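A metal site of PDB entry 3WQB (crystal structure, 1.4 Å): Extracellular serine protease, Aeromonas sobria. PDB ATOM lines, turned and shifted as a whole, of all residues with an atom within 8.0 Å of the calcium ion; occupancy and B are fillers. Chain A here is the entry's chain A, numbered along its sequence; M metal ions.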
ATOM      1  N   ILE A 452       8.529  29.939  -4.214  1.00  0.00           N
ATOM      2  CA  ILE A 452       9.928  29.908  -4.630  1.00  0.00           C
ATOM      3  C   ILE A 452      10.468  28.527  -4.272  1.00  0.00           C
ATOM      4  O   ILE A 452      10.875  28.270  -3.132  1.00  0.00           O
ATOM      5  CB  ILE A 452      10.787  31.019  -3.946  1.00  0.00           C
ATOM      6  CG1 ILE A 452      10.156  32.413  -4.121  1.00  0.00           C
ATOM      7  CG2 ILE A 452      12.217  30.990  -4.479  1.00  0.00           C
ATOM      8  CD1 ILE A 452      10.705  33.470  -3.163  1.00  0.00           C
ATOM      9  N   ALA A 453      10.439  27.618  -5.238  1.00  0.00           N
ATOM     10  CA  ALA A 453      10.905  26.257  -4.990  1.00  0.00           C
ATOM     11  C   ALA A 453      12.407  26.228  -4.748  1.00  0.00           C
ATOM     12  O   ALA A 453      13.143  27.053  -5.286  1.00  0.00           O
ATOM     13  CB  ALA A 453      10.548  25.340  -6.163  1.00  0.00           C
ATOM     14  N   ASP A 454      12.856  25.278  -3.940  1.00  0.00           N
ATOM     15  CA  ASP A 454      14.279  25.013  -3.804  1.00  0.00           C
ATOM     16  C   ASP A 454      14.817  24.666  -5.194  1.00  0.00           C
ATOM     17  O   ASP A 454      14.120  24.035  -5.997  1.00  0.00           O
ATOM     18  CB  ASP A 454      14.495  23.840  -2.861  1.00  0.00           C
ATOM     19  CG  ASP A 454      15.929  23.682  -2.407  1.00  0.00           C
ATOM     20  OD1 ASP A 454      16.709  24.660  -2.468  1.00  0.00           O
ATOM     21  OD2 ASP A 454      16.284  22.557  -1.978  1.00  0.00           O
ATOM     22  N   VAL A 455      16.040  25.109  -5.505  1.00  0.00           N
ATOM     23  CA  VAL A 455      16.697  24.826  -6.806  1.00  0.00           C
ATOM     24  C   VAL A 455      15.704  24.869  -7.974  1.00  0.00           C
ATOM     25  O   VAL A 455      15.484  23.881  -8.675  1.00  0.00           O
ATOM     26  CB  VAL A 455      17.551  23.495  -6.772  1.00  0.00           C
ATOM     27  CG1 VAL A 455      18.825  23.713  -5.990  1.00  0.00           C
ATOM     28  CG2 VAL A 455      16.764  22.273  -6.224  1.00  0.00           C
ATOM     29  N   GLY A 456      15.113  26.045  -8.187  1.00  0.00           N
ATOM     30  CA  GLY A 456      13.982  26.165  -9.096  1.00  0.00           C
ATOM     31  C   GLY A 456      14.312  25.882 -10.547  1.00  0.00           C
ATOM     32  O   GLY A 456      15.414  26.163 -11.018  1.00  0.00           O
ATOM     33  N   HIS A 483      11.918  33.085   3.056  1.00  0.00           N
ATOM     34  CA  HIS A 483      12.834  32.038   2.627  1.00  0.00           C
ATOM     35  C   HIS A 483      13.829  31.768   3.734  1.00  0.00           C
ATOM     36  O   HIS A 483      14.361  32.689   4.352  1.00  0.00           O
ATOM     37  CB  HIS A 483      13.585  32.464   1.355  1.00  0.00           C
ATOM     38  CG  HIS A 483      14.326  31.345   0.703  1.00  0.00           C
ATOM     39  ND1 HIS A 483      15.560  30.908   1.148  1.00  0.00           N
ATOM     40  CD2 HIS A 483      14.039  30.592  -0.379  1.00  0.00           C
ATOM     41  CE1 HIS A 483      15.973  29.903   0.387  1.00  0.00           C
ATOM     42  NE2 HIS A 483      15.071  29.693  -0.554  1.00  0.00           N
ATOM     43  N   GLN A 484      14.058  30.477   3.995  1.00  0.00           N
ATOM     44  CA  GLN A 484      14.854  30.043   5.135  1.00  0.00           C
ATOM     45  C   GLN A 484      16.385  30.146   4.969  1.00  0.00           C
ATOM     46  O   GLN A 484      17.112  30.026   5.944  1.00  0.00           O
ATOM     47  CB  GLN A 484      14.495  28.610   5.526  1.00  0.00           C
ATOM     48  CG  GLN A 484      13.076  28.410   6.029  1.00  0.00           C
ATOM     49  CD  GLN A 484      12.684  26.944   6.074  1.00  0.00           C
ATOM     50  OE1 GLN A 484      13.052  26.158   5.184  1.00  0.00           O
ATOM     51  NE2 GLN A 484      11.947  26.562   7.102  1.00  0.00           N
ATOM     52  N   ARG A 485      16.851  30.348   3.742  1.00  0.00           N
ATOM     53  CA  ARG A 485      18.281  30.550   3.487  1.00  0.00           C
ATOM     54  C   ARG A 485      18.505  31.634   2.430  1.00  0.00           C
ATOM     55  O   ARG A 485      18.763  31.362   1.261  1.00  0.00           O
ATOM     56  CB  ARG A 485      18.979  29.234   3.118  1.00  0.00           C
ATOM     57  CG  ARG A 485      20.492  29.359   3.027  1.00  0.00           C
ATOM     58  CD  ARG A 485      21.201  28.022   3.001  1.00  0.00           C
ATOM     59  NE  ARG A 485      21.090  27.358   1.709  1.00  0.00           N
ATOM     60  CZ  ARG A 485      21.966  26.485   1.226  1.00  0.00           C
ATOM     61  NH1 ARG A 485      23.039  26.118   1.946  1.00  0.00           N
ATOM     62  NH2 ARG A 485      21.773  25.959   0.015  1.00  0.00           N
ATOM     63  N   LEU A 486      18.407  32.879   2.878  1.00  0.00           N
ATOM     64  CA  LEU A 486      18.375  34.031   1.982  1.00  0.00           C
ATOM     65  C   LEU A 486      19.445  34.093   0.893  1.00  0.00           C
ATOM     66  O   LEU A 486      19.134  34.474  -0.229  1.00  0.00           O
ATOM     67  CB  LEU A 486      18.329  35.359   2.757  1.00  0.00           C
ATOM     68  CG  LEU A 486      17.000  35.674   3.451  1.00  0.00           C
ATOM     69  CD1 LEU A 486      17.183  36.800   4.438  1.00  0.00           C
ATOM     70  CD2 LEU A 486      15.911  36.001   2.438  1.00  0.00           C
ATOM     71  N   PRO A 487      20.706  33.721   1.213  1.00  0.00           N
ATOM     72  CA  PRO A 487      21.730  33.832   0.157  1.00  0.00           C
ATOM     73  C   PRO A 487      21.548  32.863  -1.014  1.00  0.00           C
ATOM     74  O   PRO A 487      22.251  32.981  -1.994  1.00  0.00           O
ATOM     75  CB  PRO A 487      23.043  33.566   0.905  1.00  0.00           C
ATOM     76  CG  PRO A 487      22.731  33.963   2.314  1.00  0.00           C
ATOM     77  CD  PRO A 487      21.331  33.471   2.516  1.00  0.00           C
ATOM     78  N   ASP A 488      20.577  31.944  -0.937  1.00  0.00           N
ATOM     79  CA  ASP A 488      20.235  31.124  -2.094  1.00  0.00           C
ATOM     80  C   ASP A 488      19.574  31.919  -3.219  1.00  0.00           C
ATOM     81  O   ASP A 488      19.470  31.433  -4.339  1.00  0.00           O
ATOM     82  CB  ASP A 488      19.301  29.972  -1.694  1.00  0.00           C
ATOM     83  CG  ASP A 488      20.015  28.871  -0.935  1.00  0.00           C
ATOM     84  OD1 ASP A 488      21.242  28.952  -0.768  1.00  0.00           O
ATOM     85  OD2 ASP A 488      19.318  27.918  -0.517  1.00  0.00           O
ATOM     86  N   LEU A 489      19.116  33.128  -2.913  1.00  0.00           N
ATOM     87  CA  LEU A 489      18.263  33.858  -3.839  1.00  0.00           C
ATOM     88  C   LEU A 489      19.001  34.778  -4.805  1.00  0.00           C
ATOM     89  O   LEU A 489      19.866  35.570  -4.418  1.00  0.00           O
ATOM     90  CB  LEU A 489      17.172  34.631  -3.082  1.00  0.00           C
ATOM     91  CG  LEU A 489      16.251  33.796  -2.200  1.00  0.00           C
ATOM     92  CD1 LEU A 489      15.287  34.709  -1.497  1.00  0.00           C
ATOM     93  CD2 LEU A 489      15.503  32.713  -2.984  1.00  0.00           C
ATOM     94  N   PHE A 507      24.621  34.119  -2.716  1.00  0.00           N
ATOM     95  CA  PHE A 507      25.814  33.770  -1.927  1.00  0.00           C
ATOM     96  C   PHE A 507      26.438  35.019  -1.317  1.00  0.00           C
ATOM     97  O   PHE A 507      27.636  35.099  -1.048  1.00  0.00           O
ATOM     98  CB  PHE A 507      26.832  32.936  -2.728  1.00  0.00           C
ATOM     99  CG  PHE A 507      26.199  31.808  -3.500  1.00  0.00           C
ATOM    100  CD1 PHE A 507      25.114  31.087  -2.981  1.00  0.00           C
ATOM    101  CD2 PHE A 507      26.679  31.461  -4.758  1.00  0.00           C
ATOM    102  CE1 PHE A 507      24.526  30.061  -3.710  1.00  0.00           C
ATOM    103  CE2 PHE A 507      26.095  30.426  -5.486  1.00  0.00           C
ATOM    104  CZ  PHE A 507      25.031  29.726  -4.963  1.00  0.00           C
ATOM    105  N   THR A 552      14.911  33.442  -7.904  1.00  0.00           N
ATOM    106  CA  THR A 552      15.195  32.012  -8.012  1.00  0.00           C
ATOM    107  C   THR A 552      16.058  31.557  -6.843  1.00  0.00           C
ATOM    108  O   THR A 552      17.003  32.252  -6.466  1.00  0.00           O
ATOM    109  CB  THR A 552      15.962  31.681  -9.310  1.00  0.00           C
ATOM    110  OG1 THR A 552      15.350  32.323 -10.429  1.00  0.00           O
ATOM    111  CG2 THR A 552      15.964  30.184  -9.557  1.00  0.00           C
ATOM    112  N   ASP A 553      15.728  30.402  -6.270  1.00  0.00           N
ATOM    113  CA  ASP A 553      16.604  29.717  -5.325  1.00  0.00           C
ATOM    114  C   ASP A 553      17.554  28.850  -6.147  1.00  0.00           C
ATOM    115  O   ASP A 553      17.125  27.953  -6.859  1.00  0.00           O
ATOM    116  CB  ASP A 553      15.732  28.891  -4.354  1.00  0.00           C
ATOM    117  CG  ASP A 553      16.547  28.038  -3.383  1.00  0.00           C
ATOM    118  OD1 ASP A 553      17.678  27.601  -3.682  1.00  0.00           O
ATOM    119  OD2 ASP A 553      16.029  27.764  -2.280  1.00  0.00           O
ATOM    120  N   VAL A 554      18.849  29.160  -6.072  1.00  0.00           N
ATOM    121  CA  VAL A 554      19.827  28.572  -6.980  1.00  0.00           C
ATOM    122  C   VAL A 554      20.845  27.659  -6.275  1.00  0.00           C
ATOM    123  O   VAL A 554      21.948  27.460  -6.795  1.00  0.00           O
ATOM    124  CB  VAL A 554      20.590  29.663  -7.806  1.00  0.00           C
ATOM    125  CG1 VAL A 554      19.630  30.462  -8.684  1.00  0.00           C
ATOM    126  CG2 VAL A 554      21.432  30.570  -6.912  1.00  0.00           C
ATOM    127  N   ALA A 555      20.490  27.135  -5.112  1.00  0.00           N
ATOM    128  CA  ALA A 555      21.408  26.256  -4.386  1.00  0.00           C
ATOM    129  C   ALA A 555      20.726  25.354  -3.387  1.00  0.00           C
ATOM    130  O   ALA A 555      19.853  25.794  -2.642  1.00  0.00           O
ATOM    131  CB  ALA A 555      22.477  27.079  -3.666  1.00  0.00           C
ATOM    132  N   ASN A 556      21.154  24.095  -3.351  1.00  0.00           N
ATOM    133  CA  ASN A 556      20.745  23.193  -2.280  1.00  0.00           C
ATOM    134  C   ASN A 556      21.910  22.575  -1.506  1.00  0.00           C
ATOM    135  O   ASN A 556      21.705  21.830  -0.552  1.00  0.00           O
ATOM    136  CB  ASN A 556      19.774  22.107  -2.786  1.00  0.00           C
ATOM    137  CG  ASN A 556      20.357  21.240  -3.881  1.00  0.00           C
ATOM    138  OD1 ASN A 556      21.500  21.414  -4.298  1.00  0.00           O
ATOM    139  ND2 ASN A 556      19.558  20.302  -4.360  1.00  0.00           N
ATOM    140  N   GLY A 557      23.136  22.920  -1.915  1.00  0.00           N
ATOM    141  CA  GLY A 557      24.320  22.401  -1.226  1.00  0.00           C
ATOM    142  C   GLY A 557      24.575  23.184   0.058  1.00  0.00           C
ATOM    143  O   GLY A 557      24.210  24.355   0.154  1.00  0.00           O
ATOM    144  N   ARG A 559      26.880  25.280   2.704  1.00  0.00           N
ATOM    145  CA  ARG A 559      27.985  26.212   2.604  1.00  0.00           C
ATOM    146  C   ARG A 559      28.531  26.478   3.989  1.00  0.00           C
ATOM    147  O   ARG A 559      27.796  26.390   4.976  1.00  0.00           O
ATOM    148  CB  ARG A 559      27.513  27.528   1.987  1.00  0.00           C
ATOM    149  CG  ARG A 559      27.085  27.430   0.531  1.00  0.00           C
ATOM    150  CD  ARG A 559      26.765  28.797  -0.048  1.00  0.00           C
ATOM    151  NE  ARG A 559      25.609  29.439   0.590  1.00  0.00           N
ATOM    152  CZ  ARG A 559      24.337  29.271   0.227  1.00  0.00           C
ATOM    153  NH1 ARG A 559      24.002  28.471  -0.784  1.00  0.00           N
ATOM    154  NH2 ARG A 559      23.388  29.921   0.888  1.00  0.00           N
ATOM    155  N   ARG A 577      22.542  25.771   6.345  1.00  0.00           N
ATOM    156  CA  ARG A 577      21.755  24.587   5.989  1.00  0.00           C
ATOM    157  C   ARG A 577      20.706  24.974   4.954  1.00  0.00           C
ATOM    158  O   ARG A 577      20.047  26.014   5.076  1.00  0.00           O
ATOM    159  CB  ARG A 577      21.095  24.001   7.233  1.00  0.00           C
ATOM    160  CG  ARG A 577      22.043  23.829   8.415  1.00  0.00           C
ATOM    161  CD  ARG A 577      22.655  22.433   8.456  1.00  0.00           C
ATOM    162  NE  ARG A 577      23.877  22.397   9.267  1.00  0.00           N
ATOM    163  CZ  ARG A 577      23.912  22.336  10.599  1.00  0.00           C
ATOM    164  NH1 ARG A 577      22.786  22.324  11.299  1.00  0.00           N
ATOM    165  NH2 ARG A 577      25.086  22.301  11.220  1.00  0.00           N
ATOM    166  N   ASN A 578      20.558  24.158   3.925  1.00  0.00           N
ATOM    167  CA  ASN A 578      19.554  24.411   2.903  1.00  0.00           C
ATOM    168  C   ASN A 578      18.146  24.564   3.460  1.00  0.00           C
ATOM    169  O   ASN A 578      17.784  23.917   4.443  1.00  0.00           O
ATOM    170  CB  ASN A 578      19.589  23.310   1.839  1.00  0.00           C
ATOM    171  CG  ASN A 578      18.782  23.661   0.604  1.00  0.00           C
ATOM    172  OD1 ASN A 578      18.784  24.802   0.142  1.00  0.00           O
ATOM    173  ND2 ASN A 578      18.064  22.688   0.078  1.00  0.00           N
ATOM    174  N   ASN A 579      17.354  25.460   2.862  1.00  0.00           N
ATOM    175  CA  ASN A 579      15.944  25.580   3.238  1.00  0.00           C
ATOM    176  C   ASN A 579      15.217  24.249   3.086  1.00  0.00           C
ATOM    177  O   ASN A 579      15.319  23.600   2.042  1.00  0.00           O
ATOM    178  CB  ASN A 579      15.231  26.677   2.443  1.00  0.00           C
ATOM    179  CG  ASN A 579      15.401  26.515   0.942  1.00  0.00           C
ATOM    180  OD1 ASN A 579      16.518  26.566   0.428  1.00  0.00           O
ATOM    181  ND2 ASN A 579      14.289  26.325   0.238  1.00  0.00           N
ATOM    182  N   ARG A 580      14.494  23.864   4.131  1.00  0.00           N
ATOM    183  CA  ARG A 580      13.719  22.629   4.140  1.00  0.00           C
ATOM    184  C   ARG A 580      12.403  22.768   3.357  1.00  0.00           C
ATOM    185  O   ARG A 580      11.869  21.791   2.835  1.00  0.00           O
ATOM    186  CB  ARG A 580      13.443  22.218   5.593  1.00  0.00           C
ATOM    187  CG  ARG A 580      12.697  20.913   5.747  1.00  0.00           C
ATOM    188  CD  ARG A 580      13.535  19.826   6.416  1.00  0.00           C
ATOM    189  NE  ARG A 580      12.757  18.612   6.627  1.00  0.00           N
ATOM    190  CZ  ARG A 580      11.830  18.444   7.574  1.00  0.00           C
ATOM    191  NH1 ARG A 580      11.547  19.419   8.429  1.00  0.00           N
ATOM    192  NH2 ARG A 580      11.174  17.294   7.665  1.00  0.00           N
ATOM    193  N   GLN A 581      11.875  23.991   3.309  1.00  0.00           N
ATOM    194  CA  GLN A 581      10.603  24.289   2.670  1.00  0.00           C
ATOM    195  C   GLN A 581      10.819  25.281   1.519  1.00  0.00           C
ATOM    196  O   GLN A 581      11.812  26.020   1.522  1.00  0.00           O
ATOM    197  CB  GLN A 581       9.626  24.900   3.679  1.00  0.00           C
ATOM    198  CG  GLN A 581       8.842  23.903   4.542  1.00  0.00           C
ATOM    199  CD  GLN A 581       9.659  23.266   5.661  1.00  0.00           C
ATOM    200  OE1 GLN A 581      10.303  23.961   6.459  1.00  0.00           O
ATOM    201  NE2 GLN A 581       9.608  21.950   5.754  1.00  0.00           N
HETATM  202 CA    CA M   1      17.899  26.332  -1.485  1.00  0.00          CA
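OD1 of Asp 488 lies within salt-bridge range of NH1 of Arg 559 (2.8 Å).
The backbone carbonyl oxygen (O) of Asp 488 is in hydrogen-bond range of the backbone NH (N) of Val 554, at 2.9 Å.
The guanidinium group of Arg 485 lies within salt-bridge range of the side-chain carboxylate of Asp 488, 2.9 Å away.
The backbone carbonyl oxygen (O) of Ala 555 sits close to the guanidinium group (NH2) of Arg 485 (3.3 Å).
OD1 of Asn 578 sits close to NH2 of Arg 485, at 3.2 Å.
A ring nitrogen (NE2) of His 483 sits close to the side-chain carboxylate (OD2) of Asp 553 (2.8 Å).
The backbone carbonyl oxygen (O) of Asp 553 lies within hydrogen-bond range of the backbone NH (N) of Gly 456 (3.1 Å).
The backbone carbonyl oxygen of Gln 581 lies within hydrogen-bond range of the side-chain amide nitrogen of Asn 579, at 2.8 Å.
The nearest printed residue that does not touch the calcium ion is Arg 485 (4.2 Å).
The calcium ion is bound by OD1 of Asp 454, O of Ala 555, OD2 of Asp 488, OD1 of Asn 579, OD1 of Asn 578, OD2 of Asp 553 and OD1 of Asp 553.
The calcium ion has seven donor atoms within binding distance.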
